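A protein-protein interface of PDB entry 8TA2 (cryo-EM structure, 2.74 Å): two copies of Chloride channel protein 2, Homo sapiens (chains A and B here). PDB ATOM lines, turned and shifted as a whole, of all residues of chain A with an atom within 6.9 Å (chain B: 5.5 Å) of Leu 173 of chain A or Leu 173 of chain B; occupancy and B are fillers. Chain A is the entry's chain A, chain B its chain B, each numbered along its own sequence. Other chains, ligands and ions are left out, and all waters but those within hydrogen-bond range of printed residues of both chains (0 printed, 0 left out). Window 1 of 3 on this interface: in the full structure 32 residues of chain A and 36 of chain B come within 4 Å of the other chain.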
ATOM      1  N   ALA A 158      -7.586  -5.321  -5.827  1.00  0.00           N
ATOM      2  CA  ALA A 158      -7.882  -6.606  -6.449  1.00  0.00           C
ATOM      3  C   ALA A 158      -6.682  -7.562  -6.476  1.00  0.00           C
ATOM      4  O   ALA A 158      -6.821  -8.719  -6.090  1.00  0.00           O
ATOM      5  CB  ALA A 158      -8.434  -6.331  -7.843  1.00  0.00           C
ATOM      6  N   PRO A 168      -8.152 -15.884  -7.903  1.00  0.00           N
ATOM      7  CA  PRO A 168      -7.954 -14.792  -8.853  1.00  0.00           C
ATOM      8  C   PRO A 168      -9.212 -14.049  -9.308  1.00  0.00           C
ATOM      9  O   PRO A 168      -9.103 -12.866  -9.612  1.00  0.00           O
ATOM     10  CB  PRO A 168      -7.248 -15.417 -10.054  1.00  0.00           C
ATOM     11  CG  PRO A 168      -6.476 -16.561  -9.426  1.00  0.00           C
ATOM     12  CD  PRO A 168      -7.457 -17.069  -8.385  1.00  0.00           C
ATOM     13  N   ILE A 169     -10.388 -14.679  -9.369  1.00  0.00           N
ATOM     14  CA  ILE A 169     -11.630 -13.994  -9.757  1.00  0.00           C
ATOM     15  C   ILE A 169     -12.319 -13.425  -8.520  1.00  0.00           C
ATOM     16  O   ILE A 169     -12.641 -12.240  -8.473  1.00  0.00           O
ATOM     17  CB  ILE A 169     -12.557 -14.921 -10.581  1.00  0.00           C
ATOM     18  CG1 ILE A 169     -11.813 -15.378 -11.856  1.00  0.00           C
ATOM     19  CG2 ILE A 169     -13.865 -14.192 -10.944  1.00  0.00           C
ATOM     20  CD1 ILE A 169     -12.632 -16.213 -12.839  1.00  0.00           C
ATOM     21  N   GLY A 170     -12.490 -14.231  -7.478  1.00  0.00           N
ATOM     22  CA  GLY A 170     -13.110 -13.835  -6.223  1.00  0.00           C
ATOM     23  C   GLY A 170     -12.425 -12.637  -5.566  1.00  0.00           C
ATOM     24  O   GLY A 170     -13.103 -11.758  -5.046  1.00  0.00           O
ATOM     25  N   GLY A 171     -11.100 -12.525  -5.658  1.00  0.00           N
ATOM     26  CA  GLY A 171     -10.365 -11.383  -5.130  1.00  0.00           C
ATOM     27  C   GLY A 171     -10.666 -10.055  -5.820  1.00  0.00           C
ATOM     28  O   GLY A 171     -10.624  -9.010  -5.172  1.00  0.00           O
ATOM     29  N   VAL A 172     -11.036 -10.063  -7.101  1.00  0.00           N
ATOM     30  CA  VAL A 172     -11.482  -8.860  -7.831  1.00  0.00           C
ATOM     31  C   VAL A 172     -12.894  -8.466  -7.394  1.00  0.00           C
ATOM     32  O   VAL A 172     -13.138  -7.309  -7.065  1.00  0.00           O
ATOM     33  CB  VAL A 172     -11.427  -9.066  -9.357  1.00  0.00           C
ATOM     34  CG1 VAL A 172     -11.744  -7.772 -10.112  1.00  0.00           C
ATOM     35  CG2 VAL A 172     -10.059  -9.549  -9.841  1.00  0.00           C
ATOM     36  N   LEU A 173     -13.815  -9.423  -7.312  1.00  0.00           N
ATOM     37  CA  LEU A 173     -15.202  -9.173  -6.917  1.00  0.00           C
ATOM     38  C   LEU A 173     -15.335  -8.704  -5.465  1.00  0.00           C
ATOM     39  O   LEU A 173     -16.076  -7.763  -5.199  1.00  0.00           O
ATOM     40  CB  LEU A 173     -16.052 -10.424  -7.171  1.00  0.00           C
ATOM     41  CG  LEU A 173     -16.092 -10.883  -8.638  1.00  0.00           C
ATOM     42  CD1 LEU A 173     -16.921 -12.154  -8.732  1.00  0.00           C
ATOM     43  CD2 LEU A 173     -16.700  -9.830  -9.555  1.00  0.00           C
ATOM     44  N   PHE A 174     -14.577  -9.282  -4.530  1.00  0.00           N
ATOM     45  CA  PHE A 174     -14.531  -8.832  -3.135  1.00  0.00           C
ATOM     46  C   PHE A 174     -13.978  -7.409  -3.003  1.00  0.00           C
ATOM     47  O   PHE A 174     -14.558  -6.589  -2.298  1.00  0.00           O
ATOM     48  CB  PHE A 174     -13.733  -9.851  -2.311  1.00  0.00           C
ATOM     49  CG  PHE A 174     -13.640  -9.562  -0.825  1.00  0.00           C
ATOM     50  CD1 PHE A 174     -12.613  -8.743  -0.320  1.00  0.00           C
ATOM     51  CD2 PHE A 174     -14.585 -10.116   0.056  1.00  0.00           C
ATOM     52  CE1 PHE A 174     -12.524  -8.489   1.055  1.00  0.00           C
ATOM     53  CE2 PHE A 174     -14.500  -9.853   1.433  1.00  0.00           C
ATOM     54  CZ  PHE A 174     -13.466  -9.045   1.932  1.00  0.00           C
ATOM     55  N   SER A 175     -12.914  -7.066  -3.729  1.00  0.00           N
ATOM     56  CA  SER A 175     -12.347  -5.716  -3.701  1.00  0.00           C
ATOM     57  C   SER A 175     -13.342  -4.641  -4.125  1.00  0.00           C
ATOM     58  O   SER A 175     -13.403  -3.581  -3.504  1.00  0.00           O
ATOM     59  CB  SER A 175     -11.147  -5.621  -4.626  1.00  0.00           C
ATOM     60  OG  SER A 175     -10.163  -6.502  -4.164  1.00  0.00           O
ATOM     61  N   ILE A 176     -14.160  -4.907  -5.143  1.00  0.00           N
ATOM     62  CA  ILE A 176     -15.247  -4.020  -5.550  1.00  0.00           C
ATOM     63  C   ILE A 176     -16.247  -3.874  -4.400  1.00  0.00           C
ATOM     64  O   ILE A 176     -16.501  -2.758  -3.966  1.00  0.00           O
ATOM     65  CB  ILE A 176     -15.891  -4.532  -6.856  1.00  0.00           C
ATOM     66  CG1 ILE A 176     -14.907  -4.328  -8.025  1.00  0.00           C
ATOM     67  CG2 ILE A 176     -17.221  -3.836  -7.164  1.00  0.00           C
ATOM     68  CD1 ILE A 176     -15.252  -5.134  -9.272  1.00  0.00           C
ATOM     69  N   GLU A 177     -16.785  -4.959  -3.853  1.00  0.00           N
ATOM     70  CA  GLU A 177     -17.835  -4.862  -2.844  1.00  0.00           C
ATOM     71  C   GLU A 177     -17.433  -4.155  -1.542  1.00  0.00           C
ATOM     72  O   GLU A 177     -18.287  -3.532  -0.919  1.00  0.00           O
ATOM     73  CB  GLU A 177     -18.341  -6.251  -2.491  1.00  0.00           C
ATOM     74  CG  GLU A 177     -19.072  -6.935  -3.630  1.00  0.00           C
ATOM     75  CD  GLU A 177     -19.813  -8.139  -3.074  1.00  0.00           C
ATOM     76  OE1 GLU A 177     -20.793  -7.961  -2.340  1.00  0.00           O
ATOM     77  OE2 GLU A 177     -19.491  -9.291  -3.410  1.00  0.00           O
ATOM     78  N   VAL A 178     -16.170  -4.240  -1.107  1.00  0.00           N
ATOM     79  CA  VAL A 178     -15.712  -3.607   0.145  1.00  0.00           C
ATOM     80  C   VAL A 178     -15.126  -2.214  -0.046  1.00  0.00           C
ATOM     81  O   VAL A 178     -15.277  -1.391   0.848  1.00  0.00           O
ATOM     82  CB  VAL A 178     -14.746  -4.489   0.959  1.00  0.00           C
ATOM     83  CG1 VAL A 178     -15.335  -5.869   1.199  1.00  0.00           C
ATOM     84  CG2 VAL A 178     -13.358  -4.628   0.341  1.00  0.00           C
ATOM     85  N   PHE A 183     -19.303  -0.289  -9.281  1.00  0.00           N
ATOM     86  CA  PHE A 183     -18.583  -1.266 -10.099  1.00  0.00           C
ATOM     87  C   PHE A 183     -18.363  -0.684 -11.508  1.00  0.00           C
ATOM     88  O   PHE A 183     -19.255  -0.741 -12.353  1.00  0.00           O
ATOM     89  CB  PHE A 183     -19.490  -2.522 -10.080  1.00  0.00           C
ATOM     90  CG  PHE A 183     -19.097  -3.843 -10.721  1.00  0.00           C
ATOM     91  CD1 PHE A 183     -18.358  -3.931 -11.916  1.00  0.00           C
ATOM     92  CD2 PHE A 183     -19.608  -5.023 -10.143  1.00  0.00           C
ATOM     93  CE1 PHE A 183     -18.129  -5.183 -12.511  1.00  0.00           C
ATOM     94  CE2 PHE A 183     -19.363  -6.273 -10.729  1.00  0.00           C
ATOM     95  CZ  PHE A 183     -18.628  -6.354 -11.920  1.00  0.00           C
ATOM     96  N   VAL A 185     -16.913  -1.162 -15.064  1.00  0.00           N
ATOM     97  CA  VAL A 185     -16.574  -2.357 -15.863  1.00  0.00           C
ATOM     98  C   VAL A 185     -15.126  -2.322 -16.365  1.00  0.00           C
ATOM     99  O   VAL A 185     -14.410  -3.314 -16.283  1.00  0.00           O
ATOM    100  CB  VAL A 185     -17.583  -2.534 -17.012  1.00  0.00           C
ATOM    101  CG1 VAL A 185     -17.184  -3.608 -18.025  1.00  0.00           C
ATOM    102  CG2 VAL A 185     -18.946  -2.939 -16.444  1.00  0.00           C
ATOM    103  N   TYR A 188     -12.883  -3.473 -13.448  1.00  0.00           N
ATOM    104  CA  TYR A 188     -13.056  -4.916 -13.280  1.00  0.00           C
ATOM    105  C   TYR A 188     -12.274  -5.738 -14.327  1.00  0.00           C
ATOM    106  O   TYR A 188     -11.745  -6.796 -14.009  1.00  0.00           O
ATOM    107  CB  TYR A 188     -14.557  -5.204 -13.264  1.00  0.00           C
ATOM    108  CG  TYR A 188     -14.958  -6.583 -13.716  1.00  0.00           C
ATOM    109  CD1 TYR A 188     -15.220  -6.773 -15.078  1.00  0.00           C
ATOM    110  CD2 TYR A 188     -15.101  -7.652 -12.813  1.00  0.00           C
ATOM    111  CE1 TYR A 188     -15.642  -8.023 -15.534  1.00  0.00           C
ATOM    112  CE2 TYR A 188     -15.568  -8.900 -13.272  1.00  0.00           C
ATOM    113  CZ  TYR A 188     -15.869  -9.079 -14.637  1.00  0.00           C
ATOM    114  OH  TYR A 188     -16.383 -10.244 -15.104  1.00  0.00           O
ATOM    115  N   THR A 427     -20.451  -8.555   1.853  1.00  0.00           N
ATOM    116  CA  THR A 427     -20.131  -8.992   0.500  1.00  0.00           C
ATOM    117  C   THR A 427     -20.876 -10.264   0.154  1.00  0.00           C
ATOM    118  O   THR A 427     -21.269 -10.993   1.059  1.00  0.00           O
ATOM    119  CB  THR A 427     -18.643  -9.243   0.291  1.00  0.00           C
ATOM    120  OG1 THR A 427     -18.190 -10.245   1.152  1.00  0.00           O
ATOM    121  CG2 THR A 427     -17.773  -8.037   0.553  1.00  0.00           C
ATOM    122  N   SER A 429     -19.612 -12.012  -2.929  1.00  0.00           N
ATOM    123  CA  SER A 429     -18.466 -12.612  -3.610  1.00  0.00           C
ATOM    124  C   SER A 429     -17.590 -13.546  -2.768  1.00  0.00           C
ATOM    125  O   SER A 429     -16.726 -14.213  -3.330  1.00  0.00           O
ATOM    126  CB  SER A 429     -17.595 -11.513  -4.185  1.00  0.00           C
ATOM    127  OG  SER A 429     -17.307 -10.589  -3.177  1.00  0.00           O
ATOM    128  N   THR A 430     -17.838 -13.723  -1.469  1.00  0.00           N
ATOM    129  CA  THR A 430     -17.284 -14.864  -0.726  1.00  0.00           C
ATOM    130  C   THR A 430     -17.760 -16.205  -1.278  1.00  0.00           C
ATOM    131  O   THR A 430     -17.049 -17.191  -1.131  1.00  0.00           O
ATOM    132  CB  THR A 430     -17.585 -14.806   0.771  1.00  0.00           C
ATOM    133  OG1 THR A 430     -18.968 -14.756   0.998  1.00  0.00           O
ATOM    134  CG2 THR A 430     -16.939 -13.589   1.408  1.00  0.00           C
ATOM    135  N   VAL A 432     -17.828 -16.834  -4.620  1.00  0.00           N
ATOM    136  CA  VAL A 432     -16.868 -17.066  -5.717  1.00  0.00           C
ATOM    137  C   VAL A 432     -15.493 -17.475  -5.190  1.00  0.00           C
ATOM    138  O   VAL A 432     -14.894 -18.412  -5.703  1.00  0.00           O
ATOM    139  CB  VAL A 432     -16.758 -15.826  -6.623  1.00  0.00           C
ATOM    140  CG1 VAL A 432     -15.786 -16.025  -7.789  1.00  0.00           C
ATOM    141  CG2 VAL A 432     -18.130 -15.483  -7.205  1.00  0.00           C
ATOM    142  N   ILE A 433     -15.017 -16.826  -4.117  1.00  0.00           N
ATOM    143  CA  ILE A 433     -13.758 -17.152  -3.427  1.00  0.00           C
ATOM    144  C   ILE A 433     -13.743 -18.621  -2.988  1.00  0.00           C
ATOM    145  O   ILE A 433     -12.748 -19.315  -3.181  1.00  0.00           O
ATOM    146  CB  ILE A 433     -13.548 -16.195  -2.223  1.00  0.00           C
ATOM    147  CG1 ILE A 433     -13.232 -14.770  -2.728  1.00  0.00           C
ATOM    148  CG2 ILE A 433     -12.437 -16.660  -1.264  1.00  0.00           C
ATOM    149  CD1 ILE A 433     -13.381 -13.660  -1.686  1.00  0.00           C
ATOM    150  N   ILE B 169     -24.111 -16.922 -11.238  1.00  0.00           N
ATOM    151  CA  ILE B 169     -23.204 -15.809 -10.911  1.00  0.00           C
ATOM    152  C   ILE B 169     -22.635 -15.206 -12.200  1.00  0.00           C
ATOM    153  O   ILE B 169     -22.654 -13.990 -12.384  1.00  0.00           O
ATOM    154  CB  ILE B 169     -22.100 -16.241  -9.912  1.00  0.00           C
ATOM    155  CG1 ILE B 169     -22.707 -16.875  -8.640  1.00  0.00           C
ATOM    156  CG2 ILE B 169     -21.220 -15.037  -9.552  1.00  0.00           C
ATOM    157  CD1 ILE B 169     -21.692 -17.337  -7.596  1.00  0.00           C
ATOM    158  N   GLY B 170     -22.199 -16.029 -13.150  1.00  0.00           N
ATOM    159  CA  GLY B 170     -21.656 -15.579 -14.425  1.00  0.00           C
ATOM    160  C   GLY B 170     -22.670 -14.859 -15.316  1.00  0.00           C
ATOM    161  O   GLY B 170     -22.287 -13.949 -16.044  1.00  0.00           O
ATOM    162  N   GLY B 171     -23.967 -15.172 -15.211  1.00  0.00           N
ATOM    163  CA  GLY B 171     -25.050 -14.435 -15.867  1.00  0.00           C
ATOM    164  C   GLY B 171     -25.242 -13.012 -15.333  1.00  0.00           C
ATOM    165  O   GLY B 171     -25.327 -12.068 -16.115  1.00  0.00           O
ATOM    166  N   VAL B 172     -25.215 -12.830 -14.010  1.00  0.00           N
ATOM    167  CA  VAL B 172     -25.206 -11.507 -13.354  1.00  0.00           C
ATOM    168  C   VAL B 172     -23.988 -10.686 -13.785  1.00  0.00           C
ATOM    169  O   VAL B 172     -24.133  -9.545 -14.209  1.00  0.00           O
ATOM    170  CB  VAL B 172     -25.248 -11.655 -11.821  1.00  0.00           C
ATOM    171  CG1 VAL B 172     -25.235 -10.303 -11.103  1.00  0.00           C
ATOM    172  CG2 VAL B 172     -26.494 -12.407 -11.359  1.00  0.00           C
ATOM    173  N   LEU B 173     -22.791 -11.269 -13.763  1.00  0.00           N
ATOM    174  CA  LEU B 173     -21.565 -10.579 -14.160  1.00  0.00           C
ATOM    175  C   LEU B 173     -21.527 -10.246 -15.661  1.00  0.00           C
ATOM    176  O   LEU B 173     -21.123  -9.151 -16.021  1.00  0.00           O
ATOM    177  CB  LEU B 173     -20.357 -11.428 -13.734  1.00  0.00           C
ATOM    178  CG  LEU B 173     -20.172 -11.605 -12.217  1.00  0.00           C
ATOM    179  CD1 LEU B 173     -19.051 -12.609 -11.963  1.00  0.00           C
ATOM    180  CD2 LEU B 173     -19.832 -10.289 -11.529  1.00  0.00           C
ATOM    181  N   PHE B 174     -22.001 -11.132 -16.546  1.00  0.00           N
ATOM    182  CA  PHE B 174     -22.101 -10.895 -17.997  1.00  0.00           C
ATOM    183  C   PHE B 174     -23.043  -9.738 -18.336  1.00  0.00           C
ATOM    184  O   PHE B 174     -22.700  -8.856 -19.118  1.00  0.00           O
ATOM    185  CB  PHE B 174     -22.571 -12.194 -18.666  1.00  0.00           C
ATOM    186  CG  PHE B 174     -22.759 -12.161 -20.174  1.00  0.00           C
ATOM    187  CD1 PHE B 174     -23.909 -11.589 -20.751  1.00  0.00           C
ATOM    188  CD2 PHE B 174     -21.804 -12.756 -21.009  1.00  0.00           C
ATOM    189  CE1 PHE B 174     -24.099 -11.600 -22.139  1.00  0.00           C
ATOM    190  CE2 PHE B 174     -21.991 -12.762 -22.399  1.00  0.00           C
ATOM    191  CZ  PHE B 174     -23.134 -12.180 -22.967  1.00  0.00           C
ATOM    192  N   SER B 175     -24.212  -9.697 -17.702  1.00  0.00           N
ATOM    193  CA  SER B 175     -25.203  -8.638 -17.882  1.00  0.00           C
ATOM    194  C   SER B 175     -24.643  -7.248 -17.604  1.00  0.00           C
ATOM    195  O   SER B 175     -24.865  -6.331 -18.390  1.00  0.00           O
ATOM    196  CB  SER B 175     -26.388  -8.884 -16.965  1.00  0.00           C
ATOM    197  OG  SER B 175     -26.873 -10.171 -17.222  1.00  0.00           O
ATOM    198  N   ILE B 176     -23.883  -7.093 -16.521  1.00  0.00           N
ATOM    199  CA  ILE B 176     -23.215  -5.844 -16.161  1.00  0.00           C
ATOM    200  C   ILE B 176     -22.215  -5.441 -17.249  1.00  0.00           C
ATOM    201  O   ILE B 176     -22.202  -4.288 -17.662  1.00  0.00           O
ATOM    202  CB  ILE B 176     -22.568  -5.986 -14.763  1.00  0.00           C
ATOM    203  CG1 ILE B 176     -23.655  -6.168 -13.683  1.00  0.00           C
ATOM    204  CG2 ILE B 176     -21.688  -4.782 -14.421  1.00  0.00           C
ATOM    205  CD1 ILE B 176     -23.138  -6.664 -12.333  1.00  0.00           C
ATOM    206  N   GLU B 177     -21.415  -6.368 -17.775  1.00  0.00           N
ATOM    207  CA  GLU B 177     -20.414  -6.055 -18.798  1.00  0.00           C
ATOM    208  C   GLU B 177     -21.009  -5.609 -20.137  1.00  0.00           C
ATOM    209  O   GLU B 177     -20.385  -4.811 -20.834  1.00  0.00           O
ATOM    210  CB  GLU B 177     -19.508  -7.266 -19.036  1.00  0.00           C
ATOM    211  CG  GLU B 177     -18.635  -7.578 -17.824  1.00  0.00           C
ATOM    212  CD  GLU B 177     -17.607  -8.667 -18.147  1.00  0.00           C
ATOM    213  OE1 GLU B 177     -16.711  -8.417 -18.983  1.00  0.00           O
ATOM    214  OE2 GLU B 177     -17.596  -9.723 -17.477  1.00  0.00           O
ATOM    215  N   TYR B 188     -25.954  -5.204  -8.198  1.00  0.00           N
ATOM    216  CA  TYR B 188     -25.302  -6.511  -8.248  1.00  0.00           C
ATOM    217  C   TYR B 188     -25.812  -7.450  -7.138  1.00  0.00           C
ATOM    218  O   TYR B 188     -26.105  -8.606  -7.420  1.00  0.00           O
ATOM    219  CB  TYR B 188     -23.783  -6.283  -8.271  1.00  0.00           C
ATOM    220  CG  TYR B 188     -22.926  -7.362  -7.649  1.00  0.00           C
ATOM    221  CD1 TYR B 188     -22.671  -7.288  -6.275  1.00  0.00           C
ATOM    222  CD2 TYR B 188     -22.369  -8.412  -8.408  1.00  0.00           C
ATOM    223  CE1 TYR B 188     -21.865  -8.248  -5.658  1.00  0.00           C
ATOM    224  CE2 TYR B 188     -21.536  -9.367  -7.786  1.00  0.00           C
ATOM    225  CZ  TYR B 188     -21.266  -9.274  -6.406  1.00  0.00           C
ATOM    226  OH  TYR B 188     -20.421 -10.138  -5.793  1.00  0.00           O
ATOM    227  N   SER B 429     -16.473 -12.289 -18.052  1.00  0.00           N
ATOM    228  CA  SER B 429     -17.358 -13.227 -17.339  1.00  0.00           C
ATOM    229  C   SER B 429     -17.631 -14.552 -18.072  1.00  0.00           C
ATOM    230  O   SER B 429     -18.062 -15.520 -17.451  1.00  0.00           O
ATOM    231  CB  SER B 429     -18.682 -12.554 -16.974  1.00  0.00           C
ATOM    232  OG  SER B 429     -19.486 -13.441 -16.228  1.00  0.00           O
ATOM    233  N   VAL B 432     -16.167 -17.225 -16.016  1.00  0.00           N
ATOM    234  CA  VAL B 432     -16.963 -17.648 -14.858  1.00  0.00           C
ATOM    235  C   VAL B 432     -18.108 -18.559 -15.284  1.00  0.00           C
ATOM    236  O   VAL B 432     -18.374 -19.566 -14.635  1.00  0.00           O
ATOM    237  CB  VAL B 432     -17.509 -16.431 -14.089  1.00  0.00           C
ATOM    238  CG1 VAL B 432     -18.160 -16.850 -12.771  1.00  0.00           C
ATOM    239  CG2 VAL B 432     -16.406 -15.425 -13.767  1.00  0.00           C
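The side-chain hydroxyl (OH) of Tyr 188 of chain A sits at hydrogen-bond distance from the side-chain carboxylate (OE2) of Glu 177 of chain B (2.7 Å). OE2 of Glu 177 of chain A lies within hydrogen-bond range of OH of Tyr 188 of chain B (2.7 Å).
The side-chain carboxylate (OE2) of Glu 177 of chain A sits at hydrogen-bond distance from the side-chain hydroxyl (OG) of Ser 429 of chain A (2.6 Å). OE2 of Glu 177 of chain B is in hydrogen-bond range of N of Ser 429 of chain B (2.9 Å). The side-chain hydroxyl (OG) of Ser 429 of chain B sits at hydrogen-bond distance from the backbone NH (N) of Phe 174 of chain B, 3.4 Å away. OG of Ser 429 of chain B lies within hydrogen-bond range of O of Gly 170 of chain B, at 2.9 Å. The backbone NH (N) of Phe 174 of chain A lies close to the side-chain hydroxyl (OG) of Ser 429 of chain A, at 3.3 Å.
Among the printed residues, merely in contact across the chains: Ile 169 of chain A with Val 432 of chain B (3.97 Å), Leu 173 of chain A with Leu 173 of chain B (3.7 Å), Val 185 of chain A with Ile 176 of chain B (3.7 Å), Tyr 188 of chain A with Ser 429 of chain B (3.6 Å), Ser 429 of chain A with Tyr 188 of chain B (3.5 Å) and Val 432 of chain A with Ile 169 of chain B (3.9 Å).
Gly 170 of chain A touches none of the printed residues of chain B. Of the printed residues of chain B, Tyr 188 of chain A touches Glu 177 (2.7 Å) and Ser 429 (3.6 Å). Thr 427 of chain A touches none of the printed residues of chain B. Of the printed residues of chain B, Ser 429 of chain A touches Tyr 188 (3.5 Å). Of the printed residues of chain A, Ile 169 of chain B touches Val 432. Leu 173 of chain B touches just one residue of chain A: Leu 173 (3.7 Å). Printed residues of chain A within 4 Å of Ile 176 of chain B: Val 185 (3.7 Å). The nearest residue of chain B that does not touch Leu 173 of chain A is Tyr 188 of chain B (4.6 Å). The nearest printed residue of chain A that does not touch Glu 177 of chain B is Val 185 of chain A (4.1 Å).
Of the 20 printed residues of chain A, 7 touch a printed residue of chain B. Hydrophobic or aromatic side chains of chain A within 4 Å of the printed part of chain B: Ile 169, Leu 173, Val 185, Tyr 188 and Val 432. Of the 12 printed residues of chain B, 7 touch a printed residue of chain A. Hydrophobic or aromatic side chains of chain B that line the printed part of chain A: Ile 169, Leu 173, Ile 176, Tyr 188 and Val 432. Among the printed residues, no Asp or Glu carboxylate lies within 4 Å of a Lys or Arg side-chain nitrogen of the other chain.
Ile 169 of chain A touches Val 432 of chain B, and with the chains exchanged Val 432 of chain A touches Ile 169 of chain B. Leu 173 of chain A touches its own counterpart, Leu 173 of chain B. Glu 177 of chain A touches Tyr 188 of chain B, and with the chains exchanged Tyr 188 of chain A touches Glu 177 of chain B. Tyr 188 of chain A touches Ser 429 of chain B, and with the chains exchanged Ser 429 of chain A touches Tyr 188 of chain B. Positions printed for both chains: 169, 170, 171, 172, 173, 174, 175, 176, 177, 188, 429 and 432. Of the 8 pairs that touch across the chains among the printed residues, 7 have their exchanged pair printed and touching as well.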
